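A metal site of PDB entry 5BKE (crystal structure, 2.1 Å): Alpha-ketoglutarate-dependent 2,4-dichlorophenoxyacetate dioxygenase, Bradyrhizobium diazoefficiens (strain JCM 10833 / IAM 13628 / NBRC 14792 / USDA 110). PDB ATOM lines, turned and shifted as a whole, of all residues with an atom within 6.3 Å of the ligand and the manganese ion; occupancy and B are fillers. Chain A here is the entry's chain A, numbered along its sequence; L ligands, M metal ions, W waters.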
ATOM      1  N   VAL A  88      12.015  38.097  22.815  1.00  0.00           N
ATOM      2  CA  VAL A  88      11.177  37.061  22.178  1.00  0.00           C
ATOM      3  C   VAL A  88       9.866  36.866  22.989  1.00  0.00           C
ATOM      4  O   VAL A  88       9.181  35.818  22.897  1.00  0.00           O
ATOM      5  CB  VAL A  88      11.958  35.746  21.920  1.00  0.00           C
ATOM      6  CG1 VAL A  88      13.171  35.992  21.019  1.00  0.00           C
ATOM      7  CG2 VAL A  88      12.413  35.118  23.219  1.00  0.00           C
ATOM      8  N   ASN A 111       8.496  32.162  15.229  1.00  0.00           N
ATOM      9  CA  ASN A 111       9.123  31.210  16.149  1.00  0.00           C
ATOM     10  C   ASN A 111       8.310  29.920  16.359  1.00  0.00           C
ATOM     11  O   ASN A 111       8.834  28.923  16.879  1.00  0.00           O
ATOM     12  CB  ASN A 111       9.454  31.871  17.487  1.00  0.00           C
ATOM     13  CG  ASN A 111      10.537  32.946  17.359  1.00  0.00           C
ATOM     14  OD1 ASN A 111      11.275  33.011  16.372  1.00  0.00           O
ATOM     15  ND2 ASN A 111      10.658  33.778  18.391  1.00  0.00           N
ATOM     16  N   HIS A 115      12.775  25.968  13.395  1.00  0.00           N
ATOM     17  CA  HIS A 115      13.836  26.826  12.892  1.00  0.00           C
ATOM     18  C   HIS A 115      15.123  26.644  13.686  1.00  0.00           C
ATOM     19  O   HIS A 115      15.127  26.086  14.800  1.00  0.00           O
ATOM     20  CB  HIS A 115      13.391  28.300  12.876  1.00  0.00           C
ATOM     21  CG  HIS A 115      13.255  28.917  14.243  1.00  0.00           C
ATOM     22  ND1 HIS A 115      12.124  28.773  15.013  1.00  0.00           N
ATOM     23  CD2 HIS A 115      14.126  29.654  14.967  1.00  0.00           C
ATOM     24  CE1 HIS A 115      12.300  29.407  16.166  1.00  0.00           C
ATOM     25  NE2 HIS A 115      13.514  29.956  16.161  1.00  0.00           N
ATOM     26  N   SER A 116      16.208  27.138  13.096  1.00  0.00           N
ATOM     27  CA  SER A 116      17.477  27.281  13.762  1.00  0.00           C
ATOM     28  C   SER A 116      17.825  28.767  13.704  1.00  0.00           C
ATOM     29  O   SER A 116      17.731  29.386  12.638  1.00  0.00           O
ATOM     30  CB  SER A 116      18.529  26.433  13.063  1.00  0.00           C
ATOM     31  OG  SER A 116      19.772  26.537  13.734  1.00  0.00           O
ATOM     32  N   ASP A 117      18.200  29.350  14.844  1.00  0.00           N
ATOM     33  CA  ASP A 117      18.355  30.808  14.944  1.00  0.00           C
ATOM     34  C   ASP A 117      19.394  31.392  13.975  1.00  0.00           C
ATOM     35  O   ASP A 117      20.452  30.794  13.770  1.00  0.00           O
ATOM     36  CB  ASP A 117      18.667  31.254  16.374  1.00  0.00           C
ATOM     37  CG  ASP A 117      17.482  31.052  17.323  1.00  0.00           C
ATOM     38  OD1 ASP A 117      16.322  31.022  16.877  1.00  0.00           O
ATOM     39  OD2 ASP A 117      17.751  30.928  18.533  1.00  0.00           O
ATOM     40  N   SER A 128      22.051  29.950  21.615  1.00  0.00           N
ATOM     41  CA  SER A 128      20.955  30.805  22.101  1.00  0.00           C
ATOM     42  C   SER A 128      20.574  30.399  23.522  1.00  0.00           C
ATOM     43  O   SER A 128      20.538  29.216  23.849  1.00  0.00           O
ATOM     44  CB  SER A 128      19.749  30.705  21.203  1.00  0.00           C
ATOM     45  OG  SER A 128      20.022  31.079  19.877  1.00  0.00           O
ATOM     46  N   LEU A 130      17.732  31.136  26.564  1.00  0.00           N
ATOM     47  CA  LEU A 130      16.390  31.646  26.791  1.00  0.00           C
ATOM     48  C   LEU A 130      15.967  31.528  28.254  1.00  0.00           C
ATOM     49  O   LEU A 130      15.954  30.434  28.823  1.00  0.00           O
ATOM     50  CB  LEU A 130      15.383  30.926  25.889  1.00  0.00           C
ATOM     51  CG  LEU A 130      13.956  31.465  25.799  1.00  0.00           C
ATOM     52  CD1 LEU A 130      13.957  32.914  25.318  1.00  0.00           C
ATOM     53  CD2 LEU A 130      13.099  30.599  24.886  1.00  0.00           C
ATOM     54  N   GLY A 140       2.608  27.276  24.937  1.00  0.00           N
ATOM     55  CA  GLY A 140       3.934  27.868  24.807  1.00  0.00           C
ATOM     56  C   GLY A 140       5.073  26.994  25.286  1.00  0.00           C
ATOM     57  O   GLY A 140       6.110  27.501  25.732  1.00  0.00           O
ATOM     58  N   ASN A 141       4.912  25.672  25.194  1.00  0.00           N
ATOM     59  CA  ASN A 141       6.043  24.746  25.292  1.00  0.00           C
ATOM     60  C   ASN A 141       7.084  25.055  24.212  1.00  0.00           C
ATOM     61  O   ASN A 141       6.736  25.431  23.105  1.00  0.00           O
ATOM     62  CB  ASN A 141       5.571  23.299  25.114  1.00  0.00           C
ATOM     63  CG  ASN A 141       4.736  22.792  26.282  1.00  0.00           C
ATOM     64  OD1 ASN A 141       4.605  23.460  27.323  1.00  0.00           O
ATOM     65  ND2 ASN A 141       4.168  21.598  26.121  1.00  0.00           N
ATOM     66  N   THR A 142       8.363  24.900  24.548  1.00  0.00           N
ATOM     67  CA  THR A 142       9.390  24.981  23.534  1.00  0.00           C
ATOM     68  C   THR A 142       9.873  23.576  23.225  1.00  0.00           C
ATOM     69  O   THR A 142      10.265  22.822  24.138  1.00  0.00           O
ATOM     70  CB  THR A 142      10.518  25.939  23.937  1.00  0.00           C
ATOM     71  OG1 THR A 142       9.939  27.222  24.194  1.00  0.00           O
ATOM     72  CG2 THR A 142      11.557  26.097  22.826  1.00  0.00           C
ATOM     73  N   TRP A 249       7.722  24.903  30.623  1.00  0.00           N
ATOM     74  CA  TRP A 249       8.400  26.002  31.327  1.00  0.00           C
ATOM     75  C   TRP A 249       8.001  26.132  32.803  1.00  0.00           C
ATOM     76  O   TRP A 249       6.824  26.025  33.156  1.00  0.00           O
ATOM     77  CB  TRP A 249       8.206  27.329  30.594  1.00  0.00           C
ATOM     78  CG  TRP A 249       8.931  27.392  29.270  1.00  0.00           C
ATOM     79  CD1 TRP A 249       8.405  27.135  28.044  1.00  0.00           C
ATOM     80  CD2 TRP A 249      10.309  27.741  29.062  1.00  0.00           C
ATOM     81  NE1 TRP A 249       9.369  27.286  27.072  1.00  0.00           N
ATOM     82  CE2 TRP A 249      10.547  27.657  27.671  1.00  0.00           C
ATOM     83  CE3 TRP A 249      11.367  28.103  29.910  1.00  0.00           C
ATOM     84  CZ2 TRP A 249      11.800  27.934  27.100  1.00  0.00           C
ATOM     85  CZ3 TRP A 249      12.630  28.371  29.342  1.00  0.00           C
ATOM     86  CH2 TRP A 249      12.822  28.289  27.948  1.00  0.00           C
ATOM     87  N   TRP A 257      20.595  26.379  23.815  1.00  0.00           N
ATOM     88  CA  TRP A 257      20.716  25.398  22.740  1.00  0.00           C
ATOM     89  C   TRP A 257      21.778  25.741  21.702  1.00  0.00           C
ATOM     90  O   TRP A 257      22.060  26.914  21.436  1.00  0.00           O
ATOM     91  CB  TRP A 257      19.355  25.128  22.073  1.00  0.00           C
ATOM     92  CG  TRP A 257      18.732  26.322  21.405  1.00  0.00           C
ATOM     93  CD1 TRP A 257      18.927  26.734  20.109  1.00  0.00           C
ATOM     94  CD2 TRP A 257      17.834  27.262  21.988  1.00  0.00           C
ATOM     95  NE1 TRP A 257      18.199  27.871  19.854  1.00  0.00           N
ATOM     96  CE2 TRP A 257      17.513  28.217  20.996  1.00  0.00           C
ATOM     97  CE3 TRP A 257      17.262  27.396  23.270  1.00  0.00           C
ATOM     98  CZ2 TRP A 257      16.625  29.295  21.220  1.00  0.00           C
ATOM     99  CZ3 TRP A 257      16.379  28.470  23.508  1.00  0.00           C
ATOM    100  CH2 TRP A 257      16.070  29.408  22.477  1.00  0.00           C
ATOM    101  N   ASN A 259      22.399  25.967  18.116  1.00  0.00           N
ATOM    102  CA  ASN A 259      21.681  26.111  16.850  1.00  0.00           C
ATOM    103  C   ASN A 259      22.351  25.310  15.745  1.00  0.00           C
ATOM    104  O   ASN A 259      21.724  25.005  14.737  1.00  0.00           O
ATOM    105  CB  ASN A 259      21.613  27.587  16.440  1.00  0.00           C
ATOM    106  CG  ASN A 259      20.703  28.390  17.346  1.00  0.00           C
ATOM    107  OD1 ASN A 259      19.482  28.336  17.204  1.00  0.00           O
ATOM    108  ND2 ASN A 259      21.287  29.149  18.279  1.00  0.00           N
ATOM    109  N   HIS A 264      14.328  24.246  16.878  1.00  0.00           N
ATOM    110  CA  HIS A 264      13.430  24.479  18.001  1.00  0.00           C
ATOM    111  C   HIS A 264      12.212  25.215  17.499  1.00  0.00           C
ATOM    112  O   HIS A 264      12.238  25.792  16.413  1.00  0.00           O
ATOM    113  CB  HIS A 264      14.143  25.258  19.125  1.00  0.00           C
ATOM    114  CG  HIS A 264      14.646  26.595  18.692  1.00  0.00           C
ATOM    115  ND1 HIS A 264      15.779  26.746  17.901  1.00  0.00           N
ATOM    116  CD2 HIS A 264      14.178  27.852  18.905  1.00  0.00           C
ATOM    117  CE1 HIS A 264      15.966  28.033  17.653  1.00  0.00           C
ATOM    118  NE2 HIS A 264      15.022  28.720  18.258  1.00  0.00           N
ATOM    119  N   ARG A 265      11.135  25.177  18.274  1.00  0.00           N
ATOM    120  CA  ARG A 265       9.913  25.956  18.003  1.00  0.00           C
ATOM    121  C   ARG A 265       9.128  26.162  19.286  1.00  0.00           C
ATOM    122  O   ARG A 265       9.233  25.360  20.225  1.00  0.00           O
ATOM    123  CB  ARG A 265       9.019  25.280  16.940  1.00  0.00           C
ATOM    124  CG  ARG A 265       8.366  23.982  17.385  1.00  0.00           C
ATOM    125  CD  ARG A 265       7.350  23.465  16.380  1.00  0.00           C
ATOM    126  NE  ARG A 265       6.780  22.179  16.806  1.00  0.00           N
ATOM    127  CZ  ARG A 265       5.776  21.548  16.199  1.00  0.00           C
ATOM    128  NH1 ARG A 265       5.192  22.082  15.143  1.00  0.00           N
ATOM    129  NH2 ARG A 265       5.323  20.388  16.679  1.00  0.00           N
ATOM    130  N   VAL A 266       8.347  27.237  19.322  1.00  0.00           N
ATOM    131  CA  VAL A 266       7.383  27.476  20.381  1.00  0.00           C
ATOM    132  C   VAL A 266       5.973  27.020  19.928  1.00  0.00           C
ATOM    133  O   VAL A 266       5.530  27.332  18.822  1.00  0.00           O
ATOM    134  CB  VAL A 266       7.421  28.948  20.893  1.00  0.00           C
ATOM    135  CG1 VAL A 266       7.109  29.952  19.790  1.00  0.00           C
ATOM    136  CG2 VAL A 266       6.509  29.153  22.096  1.00  0.00           C
ATOM    137  N   ARG A 267       5.287  26.267  20.789  1.00  0.00           N
ATOM    138  CA  ARG A 267       3.900  25.847  20.542  1.00  0.00           C
ATOM    139  C   ARG A 267       2.950  27.010  20.829  1.00  0.00           C
ATOM    140  O   ARG A 267       3.301  27.948  21.547  1.00  0.00           O
ATOM    141  CB  ARG A 267       3.540  24.618  21.403  1.00  0.00           C
ATOM    142  CG  ARG A 267       4.364  23.342  21.151  1.00  0.00           C
ATOM    143  CD  ARG A 267       4.688  23.054  19.684  1.00  0.00           C
ATOM    144  NE  ARG A 267       3.507  22.792  18.842  1.00  0.00           N
ATOM    145  CZ  ARG A 267       2.915  21.604  18.681  1.00  0.00           C
ATOM    146  NH1 ARG A 267       3.371  20.525  19.311  1.00  0.00           N
ATOM    147  NH2 ARG A 267       1.854  21.512  17.890  1.00  0.00           N
ATOM    148  N   TYR A 269       0.297  29.604  22.139  1.00  0.00           N
ATOM    149  CA  TYR A 269      -0.007  30.070  23.498  1.00  0.00           C
ATOM    150  C   TYR A 269      -1.094  31.146  23.495  1.00  0.00           C
ATOM    151  O   TYR A 269      -1.403  31.723  22.453  1.00  0.00           O
ATOM    152  CB  TYR A 269       1.259  30.543  24.236  1.00  0.00           C
ATOM    153  CG  TYR A 269       2.115  31.536  23.475  1.00  0.00           C
ATOM    154  CD1 TYR A 269       3.141  31.106  22.621  1.00  0.00           C
ATOM    155  CD2 TYR A 269       1.918  32.918  23.611  1.00  0.00           C
ATOM    156  CE1 TYR A 269       3.937  32.002  21.919  1.00  0.00           C
ATOM    157  CE2 TYR A 269       2.705  33.830  22.923  1.00  0.00           C
ATOM    158  CZ  TYR A 269       3.712  33.370  22.081  1.00  0.00           C
ATOM    159  OH  TYR A 269       4.498  34.276  21.377  1.00  0.00           O
ATOM    160  N   ARG A 275       3.824  36.676  28.414  1.00  0.00           N
ATOM    161  CA  ARG A 275       4.860  35.659  28.233  1.00  0.00           C
ATOM    162  C   ARG A 275       6.174  36.415  28.082  1.00  0.00           C
ATOM    163  O   ARG A 275       6.474  36.890  26.994  1.00  0.00           O
ATOM    164  CB  ARG A 275       4.589  34.804  26.972  1.00  0.00           C
ATOM    165  CG  ARG A 275       5.461  33.566  26.868  1.00  0.00           C
ATOM    166  CD  ARG A 275       5.030  32.648  25.731  1.00  0.00           C
ATOM    167  NE  ARG A 275       5.770  31.377  25.744  1.00  0.00           N
ATOM    168  CZ  ARG A 275       6.921  31.131  25.101  1.00  0.00           C
ATOM    169  NH1 ARG A 275       7.530  32.070  24.377  1.00  0.00           N
ATOM    170  NH2 ARG A 275       7.478  29.934  25.197  1.00  0.00           N
ATOM    171  N   MET A 277       9.851  36.194  27.875  1.00  0.00           N
ATOM    172  CA  MET A 277      10.987  35.346  27.531  1.00  0.00           C
ATOM    173  C   MET A 277      12.049  36.216  26.857  1.00  0.00           C
ATOM    174  O   MET A 277      11.721  37.043  25.991  1.00  0.00           O
ATOM    175  CB  MET A 277      10.553  34.225  26.590  1.00  0.00           C
ATOM    176  CG  MET A 277       9.272  33.509  27.008  1.00  0.00           C
ATOM    177  SD  MET A 277       9.406  32.503  28.505  1.00  0.00           S
ATOM    178  CE  MET A 277      10.491  31.192  27.933  1.00  0.00           C
ATOM    179  N   ARG A 278      13.299  36.037  27.278  1.00  0.00           N
ATOM    180  CA  ARG A 278      14.419  36.888  26.870  1.00  0.00           C
ATOM    181  C   ARG A 278      15.605  36.022  26.448  1.00  0.00           C
ATOM    182  O   ARG A 278      15.997  35.097  27.158  1.00  0.00           O
ATOM    183  CB  ARG A 278      14.837  37.824  28.008  1.00  0.00           C
ATOM    184  CG  ARG A 278      13.668  38.609  28.593  1.00  0.00           C
ATOM    185  CD  ARG A 278      14.103  39.699  29.533  1.00  0.00           C
ATOM    186  NE  ARG A 278      12.944  40.195  30.259  1.00  0.00           N
ATOM    187  CZ  ARG A 278      12.960  41.160  31.172  1.00  0.00           C
ATOM    188  NH1 ARG A 278      11.829  41.513  31.762  1.00  0.00           N
ATOM    189  NH2 ARG A 278      14.093  41.762  31.518  1.00  0.00           N
ATOM    190  N   ARG A 279      16.141  36.330  25.269  1.00  0.00           N
ATOM    191  CA  ARG A 279      17.173  35.513  24.659  1.00  0.00           C
ATOM    192  C   ARG A 279      18.513  36.251  24.616  1.00  0.00           C
ATOM    193  O   ARG A 279      18.563  37.451  24.344  1.00  0.00           O
ATOM    194  CB  ARG A 279      16.739  35.065  23.253  1.00  0.00           C
ATOM    195  CG  ARG A 279      17.582  33.936  22.688  1.00  0.00           C
ATOM    196  CD  ARG A 279      17.222  33.609  21.256  1.00  0.00           C
ATOM    197  NE  ARG A 279      17.846  34.503  20.282  1.00  0.00           N
ATOM    198  CZ  ARG A 279      17.418  34.699  19.044  1.00  0.00           C
ATOM    199  NH1 ARG A 279      16.327  34.086  18.592  1.00  0.00           N
ATOM    200  NH2 ARG A 279      18.068  35.534  18.236  1.00  0.00           N
HETATM  201  C1  LIG L   1      14.048  31.986  20.363  1.00  0.00           C
HETATM  202  C2  LIG L   1      12.820  31.239  20.207  1.00  0.00           C
HETATM  203  C3  LIG L   1      11.119  30.080  21.564  1.00  0.00           C
HETATM  204  C4  LIG L   1      10.149  30.469  22.649  1.00  0.00           C
HETATM  205  O1  LIG L   1      14.921  31.945  19.462  1.00  0.00           O
HETATM  206  O2  LIG L   1      14.185  32.618  21.428  1.00  0.00           O
HETATM  207  O3  LIG L   1      12.602  30.693  19.118  1.00  0.00           O
HETATM  208  O4  LIG L   1       9.830  29.581  23.475  1.00  0.00           O
HETATM  209  N1  LIG L   1      12.013  31.179  21.266  1.00  0.00           N
HETATM  210  O5  LIG L   1       9.676  31.643  22.682  1.00  0.00           O
HETATM  211 MN    MN M   1      14.412  30.733  17.853  1.00  0.00          MN
HETATM  212  O   HOH W   1      13.843  32.666  17.085  1.00  0.00           O
HETATM  213  O   HOH W   2       8.889  33.641  20.962  1.00  0.00           O
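Merely in contact with the ligand: Asn 111 (3.5 Å), Val 88 (3.5 Å), Val 266 (3.6 Å), Trp 257 (3.6 Å) and Leu 130 (3.7 Å). Hydrophobic or aromatic side chains that line the ligand: Val 88, His 115, Leu 130, Trp 257, His 264 and Val 266. Of the 22 residues printed, 11 come within 4 Å of the ligand.
The manganese ion is bound by NE2 of His 115 (2.1 Å), O1 of the ligand (2.1 Å), NE2 of His 264 (2.1 Å), water W1 (2.2 Å), OD1 of Asp 117 (2.2 Å) and O3 of the ligand (2.2 Å).
The guanidinium group (NH1) of Arg 279 lies within salt-bridge range of an oxygen (O2) of the ligand, 3.8 Å away. The guanidinium group of Arg 275 is in salt-bridge range of an oxygen (O5) of the ligand. The side-chain hydroxyl (OG1) of Thr 142 is in hydrogen-bond range of an oxygen (O4) of the ligand, 2.5 Å away.
Water W1 bridges OD1 of Asn 111 (2.7 Å) and NH1 of Arg 279 (3.2 Å). Water W2 lies within hydrogen-bond range of O5 of the ligand (2.8 Å), O of Val 88 (2.9 Å) and ND2 of Asn 111 (3.1 Å).
OD2 of Asp 117 lies within hydrogen-bond range of OG of Ser 128, 2.6 Å away. The indole nitrogen (NE1) of Trp 257 sits close to a ring nitrogen (ND1) of His 264 (3.3 Å). The backbone carbonyl oxygen (O) of Ser 128 is in hydrogen-bond range of the backbone NH (N) of Trp 257, at 2.8 Å. The backbone carbonyl oxygen (O) of Met 277 sits at hydrogen-bond distance from the backbone NH (N) of Val 88 (3.4 Å). The backbone NH of Asp 117 lies within hydrogen-bond range of the side-chain amide oxygen of Asn 259. The side-chain amide oxygen (OD1) of Asn 259 sits at hydrogen-bond distance from the indole nitrogen (NE1) of Trp 257, at 3.0 Å. The side-chain carboxylate (OD2) of Asp 117 sits close to the indole nitrogen (NE1) of Trp 257, at 3.4 Å. OD2 of Asp 117 is in salt-bridge range of NH1 of Arg 279 (3.5 Å).
Arg 279 touches the manganese ion. Within 4 Å of the manganese ion: His 115, Asp 117, His 264 and Arg 279. The nearest printed residue that does not touch the manganese ion is Asn 111 (4.2 Å).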
